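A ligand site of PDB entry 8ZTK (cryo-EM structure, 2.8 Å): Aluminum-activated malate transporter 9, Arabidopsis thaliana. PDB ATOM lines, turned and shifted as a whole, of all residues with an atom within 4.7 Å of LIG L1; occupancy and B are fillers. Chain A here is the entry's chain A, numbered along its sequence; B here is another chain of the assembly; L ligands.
NH1 of Arg 143 is in salt-bridge range of O3 of LIG L1 (3.6 Å). O1 of LIG L1 is in salt-bridge range of NH1 of Arg 200 of chain A (3.1 Å). The guanidinium group (NH1) of Arg 200 of chain B lies within salt-bridge range of an oxygen (O1) of LG2 L2 (3.2 Å).
The side-chain hydroxyl (OG1) of Thr 147 is in hydrogen-bond range of the backbone carbonyl oxygen (O) of Arg 143 (3.4 Å). The backbone carbonyl oxygen of Trp 120 lies within hydrogen-bond range of the side-chain hydroxyl of Thr 124. O of Val 201 is in hydrogen-bond range of OG1 of Thr 205 (2.9 Å).
Residues that only touch LIG L1: Trp 120, Leu 123 of chain A, Thr 124, Val 127, Thr 147, Gly 151, Val 201, Leu 204, Thr 205, Tyr 208 and Phe 227. Hydrophobic or aromatic side chains that line LIG L1: Trp 120, Leu 123 of chain A, Val 127, Val 201, Leu 204, Tyr 208 and Phe 227. Along chain A the residues within 4 Å of LIG L1 span positions 120 to 227.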
ATOM      1  N   TRP A 120     -23.467 -22.960  26.011  1.00  0.00           N
ATOM      2  CA  TRP A 120     -22.421 -22.076  26.521  1.00  0.00           C
ATOM      3  C   TRP A 120     -22.627 -21.720  27.988  1.00  0.00           C
ATOM      4  O   TRP A 120     -21.654 -21.576  28.733  1.00  0.00           O
ATOM      5  CB  TRP A 120     -22.357 -20.805  25.669  1.00  0.00           C
ATOM      6  CG  TRP A 120     -21.976 -21.069  24.245  1.00  0.00           C
ATOM      7  CD1 TRP A 120     -22.820 -21.273  23.190  1.00  0.00           C
ATOM      8  CD2 TRP A 120     -20.648 -21.166  23.717  1.00  0.00           C
ATOM      9  NE1 TRP A 120     -22.099 -21.489  22.037  1.00  0.00           N
ATOM     10  CE2 TRP A 120     -20.763 -21.416  22.332  1.00  0.00           C
ATOM     11  CE3 TRP A 120     -19.367 -21.047  24.273  1.00  0.00           C
ATOM     12  CZ2 TRP A 120     -19.654 -21.572  21.508  1.00  0.00           C
ATOM     13  CZ3 TRP A 120     -18.272 -21.194  23.452  1.00  0.00           C
ATOM     14  CH2 TRP A 120     -18.416 -21.449  22.080  1.00  0.00           C
ATOM     15  N   LEU A 123     -21.415 -24.713  29.909  1.00  0.00           N
ATOM     16  CA  LEU A 123     -19.966 -24.771  29.944  1.00  0.00           C
ATOM     17  C   LEU A 123     -19.392 -23.762  30.929  1.00  0.00           C
ATOM     18  O   LEU A 123     -18.482 -24.072  31.702  1.00  0.00           O
ATOM     19  CB  LEU A 123     -19.396 -24.541  28.539  1.00  0.00           C
ATOM     20  CG  LEU A 123     -17.898 -24.784  28.345  1.00  0.00           C
ATOM     21  CD1 LEU A 123     -17.625 -26.262  28.099  1.00  0.00           C
ATOM     22  CD2 LEU A 123     -17.380 -23.944  27.196  1.00  0.00           C
ATOM     23  N   THR A 124     -19.927 -22.531  30.933  1.00  0.00           N
ATOM     24  CA  THR A 124     -19.458 -21.534  31.889  1.00  0.00           C
ATOM     25  C   THR A 124     -19.709 -21.982  33.322  1.00  0.00           C
ATOM     26  O   THR A 124     -18.817 -21.887  34.176  1.00  0.00           O
ATOM     27  CB  THR A 124     -20.150 -20.199  31.619  1.00  0.00           C
ATOM     28  OG1 THR A 124     -20.146 -19.924  30.217  1.00  0.00           O
ATOM     29  CG2 THR A 124     -19.443 -19.068  32.349  1.00  0.00           C
ATOM     30  N   VAL A 127     -17.204 -24.555  34.325  1.00  0.00           N
ATOM     31  CA  VAL A 127     -15.797 -24.176  34.286  1.00  0.00           C
ATOM     32  C   VAL A 127     -15.416 -23.141  35.343  1.00  0.00           C
ATOM     33  O   VAL A 127     -14.281 -23.167  35.823  1.00  0.00           O
ATOM     34  CB  VAL A 127     -15.420 -23.680  32.872  1.00  0.00           C
ATOM     35  CG1 VAL A 127     -14.122 -22.888  32.921  1.00  0.00           C
ATOM     36  CG2 VAL A 127     -15.287 -24.861  31.917  1.00  0.00           C
ATOM     37  N   VAL A 128     -16.326 -22.235  35.720  1.00  0.00           N
ATOM     38  CA  VAL A 128     -15.949 -21.147  36.623  1.00  0.00           C
ATOM     39  C   VAL A 128     -16.166 -21.460  38.097  1.00  0.00           C
ATOM     40  O   VAL A 128     -15.856 -20.617  38.943  1.00  0.00           O
ATOM     41  CB  VAL A 128     -16.702 -19.848  36.272  1.00  0.00           C
ATOM     42  CG1 VAL A 128     -16.444 -19.459  34.826  1.00  0.00           C
ATOM     43  CG2 VAL A 128     -18.193 -19.998  36.531  1.00  0.00           C
ATOM     44  N   GLY A 140     -11.310 -15.971  37.641  1.00  0.00           N
ATOM     45  CA  GLY A 140     -12.184 -15.201  36.766  1.00  0.00           C
ATOM     46  C   GLY A 140     -11.504 -13.955  36.249  1.00  0.00           C
ATOM     47  O   GLY A 140     -11.634 -13.599  35.067  1.00  0.00           O
ATOM     48  N   ARG A 143      -9.058 -15.168  33.485  1.00  0.00           N
ATOM     49  CA  ARG A 143      -9.757 -15.547  32.267  1.00  0.00           C
ATOM     50  C   ARG A 143     -10.346 -14.339  31.543  1.00  0.00           C
ATOM     51  O   ARG A 143     -10.388 -14.322  30.305  1.00  0.00           O
ATOM     52  CB  ARG A 143     -10.850 -16.563  32.594  1.00  0.00           C
ATOM     53  CG  ARG A 143     -10.329 -17.940  32.920  1.00  0.00           C
ATOM     54  CD  ARG A 143     -11.462 -18.929  33.135  1.00  0.00           C
ATOM     55  NE  ARG A 143     -11.363 -19.581  34.438  1.00  0.00           N
ATOM     56  CZ  ARG A 143     -10.994 -20.837  34.624  1.00  0.00           C
ATOM     57  NH1 ARG A 143     -10.670 -21.620  33.595  1.00  0.00           N
ATOM     58  NH2 ARG A 143     -10.943 -21.328  35.855  1.00  0.00           N
ATOM     59  N   ALA A 144     -10.721 -13.285  32.276  1.00  0.00           N
ATOM     60  CA  ALA A 144     -11.247 -12.112  31.594  1.00  0.00           C
ATOM     61  C   ALA A 144     -10.139 -11.294  30.952  1.00  0.00           C
ATOM     62  O   ALA A 144     -10.320 -10.789  29.828  1.00  0.00           O
ATOM     63  CB  ALA A 144     -12.044 -11.254  32.571  1.00  0.00           C
ATOM     64  N   THR A 147      -9.333 -13.373  27.671  1.00  0.00           N
ATOM     65  CA  THR A 147     -10.320 -13.197  26.610  1.00  0.00           C
ATOM     66  C   THR A 147     -10.305 -11.788  26.029  1.00  0.00           C
ATOM     67  O   THR A 147     -10.461 -11.621  24.811  1.00  0.00           O
ATOM     68  CB  THR A 147     -11.717 -13.524  27.139  1.00  0.00           C
ATOM     69  OG1 THR A 147     -11.864 -14.945  27.293  1.00  0.00           O
ATOM     70  CG2 THR A 147     -12.786 -13.005  26.188  1.00  0.00           C
ATOM     71  N   GLY A 151      -9.409 -10.920  22.068  1.00  0.00           N
ATOM     72  CA  GLY A 151     -10.275 -10.167  21.180  1.00  0.00           C
ATOM     73  C   GLY A 151      -9.662  -8.847  20.723  1.00  0.00           C
ATOM     74  O   GLY A 151      -9.920  -8.415  19.595  1.00  0.00           O
ATOM     75  N   GLY A 152      -8.741  -8.295  21.512  1.00  0.00           N
ATOM     76  CA  GLY A 152      -8.094  -7.057  21.141  1.00  0.00           C
ATOM     77  C   GLY A 152      -7.057  -7.254  20.069  1.00  0.00           C
ATOM     78  O   GLY A 152      -7.057  -6.527  19.071  1.00  0.00           O
ATOM     79  N   TYR A 197      -4.428 -21.524  32.194  1.00  0.00           N
ATOM     80  CA  TYR A 197      -5.806 -21.276  31.830  1.00  0.00           C
ATOM     81  C   TYR A 197      -6.042 -19.842  31.380  1.00  0.00           C
ATOM     82  O   TYR A 197      -7.142 -19.540  30.899  1.00  0.00           O
ATOM     83  CB  TYR A 197      -6.731 -21.601  33.007  1.00  0.00           C
ATOM     84  CG  TYR A 197      -6.438 -20.778  34.243  1.00  0.00           C
ATOM     85  CD1 TYR A 197      -5.359 -21.083  35.067  1.00  0.00           C
ATOM     86  CD2 TYR A 197      -7.220 -19.683  34.569  1.00  0.00           C
ATOM     87  CE1 TYR A 197      -5.091 -20.336  36.186  1.00  0.00           C
ATOM     88  CE2 TYR A 197      -6.953 -18.926  35.692  1.00  0.00           C
ATOM     89  CZ  TYR A 197      -5.881 -19.257  36.499  1.00  0.00           C
ATOM     90  OH  TYR A 197      -5.606 -18.508  37.611  1.00  0.00           O
ATOM     91  N   ARG A 200      -4.684 -20.628  27.565  1.00  0.00           N
ATOM     92  CA  ARG A 200      -5.560 -21.454  26.742  1.00  0.00           C
ATOM     93  C   ARG A 200      -6.753 -20.636  26.236  1.00  0.00           C
ATOM     94  O   ARG A 200      -7.150 -20.767  25.074  1.00  0.00           O
ATOM     95  CB  ARG A 200      -6.026 -22.672  27.521  1.00  0.00           C
ATOM     96  CG  ARG A 200      -7.306 -23.305  27.011  1.00  0.00           C
ATOM     97  CD  ARG A 200      -7.364 -24.783  27.334  1.00  0.00           C
ATOM     98  NE  ARG A 200      -6.046 -25.401  27.298  1.00  0.00           N
ATOM     99  CZ  ARG A 200      -5.657 -26.383  28.096  1.00  0.00           C
ATOM    100  NH1 ARG A 200      -6.462 -26.892  29.017  1.00  0.00           N
ATOM    101  NH2 ARG A 200      -4.422 -26.864  27.971  1.00  0.00           N
ATOM    102  N   VAL A 201      -7.314 -19.776  27.092  1.00  0.00           N
ATOM    103  CA  VAL A 201      -8.446 -18.964  26.668  1.00  0.00           C
ATOM    104  C   VAL A 201      -8.002 -17.926  25.646  1.00  0.00           C
ATOM    105  O   VAL A 201      -8.723 -17.635  24.690  1.00  0.00           O
ATOM    106  CB  VAL A 201      -9.128 -18.305  27.885  1.00  0.00           C
ATOM    107  CG1 VAL A 201     -10.060 -19.285  28.572  1.00  0.00           C
ATOM    108  CG2 VAL A 201      -8.077 -17.772  28.857  1.00  0.00           C
ATOM    109  N   LEU A 204      -7.648 -19.857  22.317  1.00  0.00           N
ATOM    110  CA  LEU A 204      -8.957 -20.240  21.788  1.00  0.00           C
ATOM    111  C   LEU A 204      -9.713 -19.020  21.267  1.00  0.00           C
ATOM    112  O   LEU A 204     -10.439 -19.117  20.273  1.00  0.00           O
ATOM    113  CB  LEU A 204      -9.771 -20.953  22.870  1.00  0.00           C
ATOM    114  CG  LEU A 204      -9.376 -22.398  23.140  1.00  0.00           C
ATOM    115  CD1 LEU A 204      -9.964 -22.876  24.466  1.00  0.00           C
ATOM    116  CD2 LEU A 204      -9.806 -23.308  21.998  1.00  0.00           C
ATOM    117  N   THR A 205      -9.570 -17.872  21.931  1.00  0.00           N
ATOM    118  CA  THR A 205     -10.314 -16.689  21.487  1.00  0.00           C
ATOM    119  C   THR A 205      -9.707 -16.133  20.211  1.00  0.00           C
ATOM    120  O   THR A 205     -10.435 -15.802  19.262  1.00  0.00           O
ATOM    121  CB  THR A 205     -10.330 -15.637  22.601  1.00  0.00           C
ATOM    122  OG1 THR A 205     -10.985 -16.163  23.759  1.00  0.00           O
ATOM    123  CG2 THR A 205     -11.067 -14.395  22.141  1.00  0.00           C
ATOM    124  N   TYR A 208     -10.618 -18.364  17.214  1.00  0.00           N
ATOM    125  CA  TYR A 208     -12.039 -18.357  16.871  1.00  0.00           C
ATOM    126  C   TYR A 208     -12.501 -17.078  16.160  1.00  0.00           C
ATOM    127  O   TYR A 208     -13.584 -17.097  15.568  1.00  0.00           O
ATOM    128  CB  TYR A 208     -12.874 -18.584  18.136  1.00  0.00           C
ATOM    129  CG  TYR A 208     -14.283 -18.002  18.120  1.00  0.00           C
ATOM    130  CD1 TYR A 208     -14.504 -16.631  18.248  1.00  0.00           C
ATOM    131  CD2 TYR A 208     -15.380 -18.823  17.946  1.00  0.00           C
ATOM    132  CE1 TYR A 208     -15.778 -16.117  18.219  1.00  0.00           C
ATOM    133  CE2 TYR A 208     -16.661 -18.307  17.910  1.00  0.00           C
ATOM    134  CZ  TYR A 208     -16.853 -16.949  18.048  1.00  0.00           C
ATOM    135  OH  TYR A 208     -18.128 -16.435  18.019  1.00  0.00           O
ATOM    136  N   ALA A 223     -21.717 -13.799  18.047  1.00  0.00           N
ATOM    137  CA  ALA A 223     -20.774 -13.444  19.098  1.00  0.00           C
ATOM    138  C   ALA A 223     -21.505 -12.815  20.281  1.00  0.00           C
ATOM    139  O   ALA A 223     -21.226 -13.131  21.443  1.00  0.00           O
ATOM    140  CB  ALA A 223     -19.697 -12.511  18.554  1.00  0.00           C
ATOM    141  N   PHE A 227     -21.686 -14.370  24.079  1.00  0.00           N
ATOM    142  CA  PHE A 227     -21.186 -13.633  25.238  1.00  0.00           C
ATOM    143  C   PHE A 227     -22.286 -13.396  26.254  1.00  0.00           C
ATOM    144  O   PHE A 227     -22.024 -13.414  27.474  1.00  0.00           O
ATOM    145  CB  PHE A 227     -20.572 -12.309  24.798  1.00  0.00           C
ATOM    146  CG  PHE A 227     -19.951 -11.537  25.919  1.00  0.00           C
ATOM    147  CD1 PHE A 227     -18.716 -11.897  26.420  1.00  0.00           C
ATOM    148  CD2 PHE A 227     -20.590 -10.442  26.465  1.00  0.00           C
ATOM    149  CE1 PHE A 227     -18.135 -11.182  27.460  1.00  0.00           C
ATOM    150  CE2 PHE A 227     -20.023  -9.723  27.491  1.00  0.00           C
ATOM    151  CZ  PHE A 227     -18.795 -10.095  27.995  1.00  0.00           C
ATOM    152  N   ILE A 230     -22.659 -16.578  28.210  1.00  0.00           N
ATOM    153  CA  ILE A 230     -21.511 -16.793  29.081  1.00  0.00           C
ATOM    154  C   ILE A 230     -21.593 -15.889  30.315  1.00  0.00           C
ATOM    155  O   ILE A 230     -21.299 -16.318  31.438  1.00  0.00           O
ATOM    156  CB  ILE A 230     -20.206 -16.571  28.304  1.00  0.00           C
ATOM    157  CG1 ILE A 230     -20.036 -17.632  27.220  1.00  0.00           C
ATOM    158  CG2 ILE A 230     -19.012 -16.566  29.245  1.00  0.00           C
ATOM    159  CD1 ILE A 230     -18.918 -17.344  26.244  1.00  0.00           C
ATOM    160  N   ALA A 234     -21.822 -17.146  34.261  1.00  0.00           N
ATOM    161  CA  ALA A 234     -20.857 -16.731  35.265  1.00  0.00           C
ATOM    162  C   ALA A 234     -21.530 -16.009  36.422  1.00  0.00           C
ATOM    163  O   ALA A 234     -21.153 -16.197  37.586  1.00  0.00           O
ATOM    164  CB  ALA A 234     -19.777 -15.861  34.625  1.00  0.00           C
ATOM    165  N   LEU B 123     -11.248 -26.221  19.119  1.00  0.00           N
ATOM    166  CA  LEU B 123     -11.257 -26.650  20.505  1.00  0.00           C
ATOM    167  C   LEU B 123     -10.669 -28.044  20.669  1.00  0.00           C
ATOM    168  O   LEU B 123      -9.876 -28.289  21.583  1.00  0.00           O
ATOM    169  CB  LEU B 123     -12.678 -26.593  21.055  1.00  0.00           C
ATOM    170  CG  LEU B 123     -12.854 -26.784  22.572  1.00  0.00           C
ATOM    171  CD1 LEU B 123     -12.622 -25.478  23.301  1.00  0.00           C
ATOM    172  CD2 LEU B 123     -14.224 -27.350  22.876  1.00  0.00           C
ATOM    173  N   ARG B 200     -15.465 -34.454  33.835  1.00  0.00           N
ATOM    174  CA  ARG B 200     -15.945 -33.188  33.314  1.00  0.00           C
ATOM    175  C   ARG B 200     -16.635 -33.372  31.961  1.00  0.00           C
ATOM    176  O   ARG B 200     -17.678 -32.765  31.700  1.00  0.00           O
ATOM    177  CB  ARG B 200     -14.794 -32.197  33.212  1.00  0.00           C
ATOM    178  CG  ARG B 200     -15.037 -31.064  32.230  1.00  0.00           C
ATOM    179  CD  ARG B 200     -14.244 -29.824  32.619  1.00  0.00           C
ATOM    180  NE  ARG B 200     -14.151 -29.679  34.064  1.00  0.00           N
ATOM    181  CZ  ARG B 200     -13.093 -29.177  34.696  1.00  0.00           C
ATOM    182  NH1 ARG B 200     -12.032 -28.743  34.032  1.00  0.00           N
ATOM    183  NH2 ARG B 200     -13.103 -29.087  36.022  1.00  0.00           N
HETATM  184  P1  LIG L   1     -10.377 -24.829  30.045  1.00  0.00           P
HETATM  185  O1  LIG L   1      -9.221 -25.604  29.449  1.00  0.00           O
HETATM  186  O2  LIG L   1     -11.118 -25.708  31.026  1.00  0.00           O
HETATM  187  O3  LIG L   1      -9.861 -23.607  30.751  1.00  0.00           O
HETATM  188  O4  LIG L   1     -11.418 -24.375  28.824  1.00  0.00           O
HETATM  189  C1  LIG L   1     -11.638 -23.003  28.615  1.00  0.00           C
HETATM  190  C2  LIG L   1     -12.681 -22.822  27.510  1.00  0.00           C
HETATM  191  C3  LIG L   1     -14.083 -22.640  28.156  1.00  0.00           C
HETATM  192  O5  LIG L   1     -12.335 -21.715  26.741  1.00  0.00           O
HETATM  193  O6  LIG L   1     -14.282 -21.295  28.574  1.00  0.00           O
HETATM  194  C4  LIG L   1     -13.393 -21.181  25.960  1.00  0.00           C
HETATM  195  O7  LIG L   1     -13.981 -21.875  25.197  1.00  0.00           O
HETATM  196  C5  LIG L   1     -13.778 -19.689  26.133  1.00  0.00           C
HETATM  197  C6  LIG L   1     -13.454 -18.894  24.830  1.00  0.00           C
HETATM  198  C7  LIG L   1     -14.625 -17.905  24.534  1.00  0.00           C
HETATM  199  C8  LIG L   1     -15.838 -18.686  23.936  1.00  0.00           C
HETATM  200  C9  LIG L   1     -15.795 -18.649  22.370  1.00  0.00           C
HETATM  201  C10 LIG L   1     -16.664 -17.477  21.830  1.00  0.00           C
HETATM  202  C11 LIG L   1     -15.840 -16.152  21.792  1.00  0.00           C
HETATM  203  C12 LIG L   1     -16.246 -15.235  22.978  1.00  0.00           C
HETATM  204  C13 LIG L   1     -17.400 -14.284  22.549  1.00  0.00           C
HETATM  205  C14 LIG L   1     -17.231 -12.901  23.266  1.00  0.00           C
HETATM  206  C15 LIG L   1     -16.031 -12.117  22.636  1.00  0.00           C
HETATM  207  C16 LIG L   1     -15.034 -11.700  23.784  1.00  0.00           C
HETATM  208  C17 LIG L   1     -13.870 -10.843  23.186  1.00  0.00           C
HETATM  209  C18 LIG L   1     -14.391  -9.419  22.817  1.00  0.00           C
HETATM  210  C19 LIG L   1     -13.209  -8.437  22.652  1.00  0.00           C
HETATM  211  C20 LIG L   1     -15.628 -21.003  28.938  1.00  0.00           C
HETATM  212  O8  LIG L   1     -16.515 -21.166  28.158  1.00  0.00           O
HETATM  213  C21 LIG L   1     -15.953 -20.452  30.358  1.00  0.00           C
HETATM  214  C22 LIG L   1     -14.878 -19.409  30.774  1.00  0.00           C
HETATM  215  C23 LIG L   1     -14.902 -18.217  29.810  1.00  0.00           C
HETATM  216  C24 LIG L   1     -13.841 -17.188  30.236  1.00  0.00           C
HETATM  217  C25 LIG L   1     -14.499 -15.847  30.621  1.00  0.00           C
HETATM  218  C26 LIG L   1     -15.258 -15.995  31.967  1.00  0.00           C
HETATM  219  C27 LIG L   1     -14.841 -14.892  32.982  1.00  0.00           C
HETATM  220  C28 LIG L   1     -16.115 -14.159  33.508  1.00  0.00           C
HETATM  221  C29 LIG L   1     -15.745 -13.328  34.786  1.00  0.00           C
HETATM  222  C30 LIG L   1     -16.206 -11.839  34.597  1.00  0.00           C
HETATM  223  C31 LIG L   1     -15.577 -10.960  35.717  1.00  0.00           C
HETATM  224  C32 LIG L   1     -15.130  -9.604  35.120  1.00  0.00           C
HETATM  225  C33 LIG L   1     -14.302  -8.834  36.163  1.00  0.00           C
HETATM  226  C34 LIG L   1     -13.626  -7.633  35.502  1.00  0.00           C
HETATM  227  C35 LIG L   1     -13.583  -6.463  36.494  1.00  0.00           C
HETATM  228  P1  LG2 L   2     -11.668 -29.624  29.480  1.00  0.00           P
HETATM  229  O1  LG2 L   2     -12.069 -29.081  30.828  1.00  0.00           O
HETATM  230  O2  LG2 L   2     -10.422 -28.917  29.012  1.00  0.00           O
HETATM  231  O3  LG2 L   2     -11.382 -31.103  29.601  1.00  0.00           O
HETATM  232  O4  LG2 L   2     -12.896 -29.378  28.393  1.00  0.00           O
HETATM  233  C1  LG2 L   2     -13.601 -30.486  27.902  1.00  0.00           C
HETATM  234  C2  LG2 L   2     -14.618 -30.031  26.863  1.00  0.00           C
HETATM  235  C3  LG2 L   2     -13.936 -29.966  25.478  1.00  0.00           C
HETATM  236  O5  LG2 L   2     -15.690 -30.926  26.842  1.00  0.00           O
HETATM  237  O6  LG2 L   2     -13.952 -31.254  24.857  1.00  0.00           O
HETATM  238  C4  LG2 L   2     -16.541 -30.780  25.721  1.00  0.00           C
HETATM  239  O7  LG2 L   2     -17.006 -29.718  25.451  1.00  0.00           O
HETATM  240  C5  LG2 L   2     -16.862 -32.023  24.840  1.00  0.00           C
HETATM  241  C6  LG2 L   2     -18.276 -32.576  25.193  1.00  0.00           C
HETATM  242  C7  LG2 L   2     -19.180 -32.558  23.922  1.00  0.00           C
HETATM  243  C8  LG2 L   2     -19.358 -31.086  23.426  1.00  0.00           C
HETATM  244  C9  LG2 L   2     -20.817 -30.882  22.881  1.00  0.00           C
HETATM  245  C10 LG2 L   2     -21.054 -31.804  21.657  1.00  0.00           C
HETATM  246  C11 LG2 L   2     -21.984 -33.010  22.018  1.00  0.00           C
HETATM  247  C12 LG2 L   2     -21.312 -34.351  21.634  1.00  0.00           C
HETATM  248  C13 LG2 L   2     -21.680 -34.702  20.164  1.00  0.00           C
HETATM  249  C14 LG2 L   2     -21.285 -36.178  19.854  1.00  0.00           C
HETATM  250  C15 LG2 L   2     -22.267 -37.155  20.593  1.00  0.00           C
HETATM  251  C16 LG2 L   2     -21.454 -38.009  21.647  1.00  0.00           C
HETATM  252  C17 LG2 L   2     -22.431 -38.961  22.433  1.00  0.00           C
HETATM  253  C18 LG2 L   2     -23.033 -40.027  21.458  1.00  0.00           C
HETATM  254  C19 LG2 L   2     -23.642 -41.194  22.267  1.00  0.00           C
HETATM  255  C20 LG2 L   2     -13.622 -31.232  23.465  1.00  0.00           C
HETATM  256  O8  LG2 L   2     -14.272 -30.574  22.706  1.00  0.00           O
HETATM  257  C21 LG2 L   2     -12.418 -32.060  22.934  1.00  0.00           C
HETATM  258  C22 LG2 L   2     -12.462 -33.492  23.521  1.00  0.00           C
HETATM  259  C23 LG2 L   2     -13.706 -34.235  22.995  1.00  0.00           C
HETATM  260  C24 LG2 L   2     -13.742 -35.665  23.576  1.00  0.00           C
HETATM  261  C25 LG2 L   2     -13.310 -36.699  22.514  1.00  0.00           C
HETATM  262  C26 LG2 L   2     -11.771 -36.664  22.313  1.00  0.00           C
HETATM  263  C27 LG2 L   2     -11.205 -38.117  22.248  1.00  0.00           C
HETATM  264  C28 LG2 L   2     -11.631 -38.788  20.904  1.00  0.00           C
HETATM  265  C29 LG2 L   2     -10.564 -39.873  20.528  1.00  0.00           C
HETATM  266  C30 LG2 L   2     -11.092 -40.751  19.350  1.00  0.00           C
HETATM  267  C31 LG2 L   2     -10.609 -42.219  19.539  1.00  0.00           C
HETATM  268  C32 LG2 L   2     -11.712 -43.030  20.251  1.00  0.00           C
HETATM  269  C33 LG2 L   2     -11.127 -44.344  20.826  1.00  0.00           C
HETATM  270  C34 LG2 L   2     -11.497 -45.515  19.916  1.00  0.00           C
HETATM  271  C35 LG2 L   2     -11.097 -46.825  20.593  1.00  0.00           C
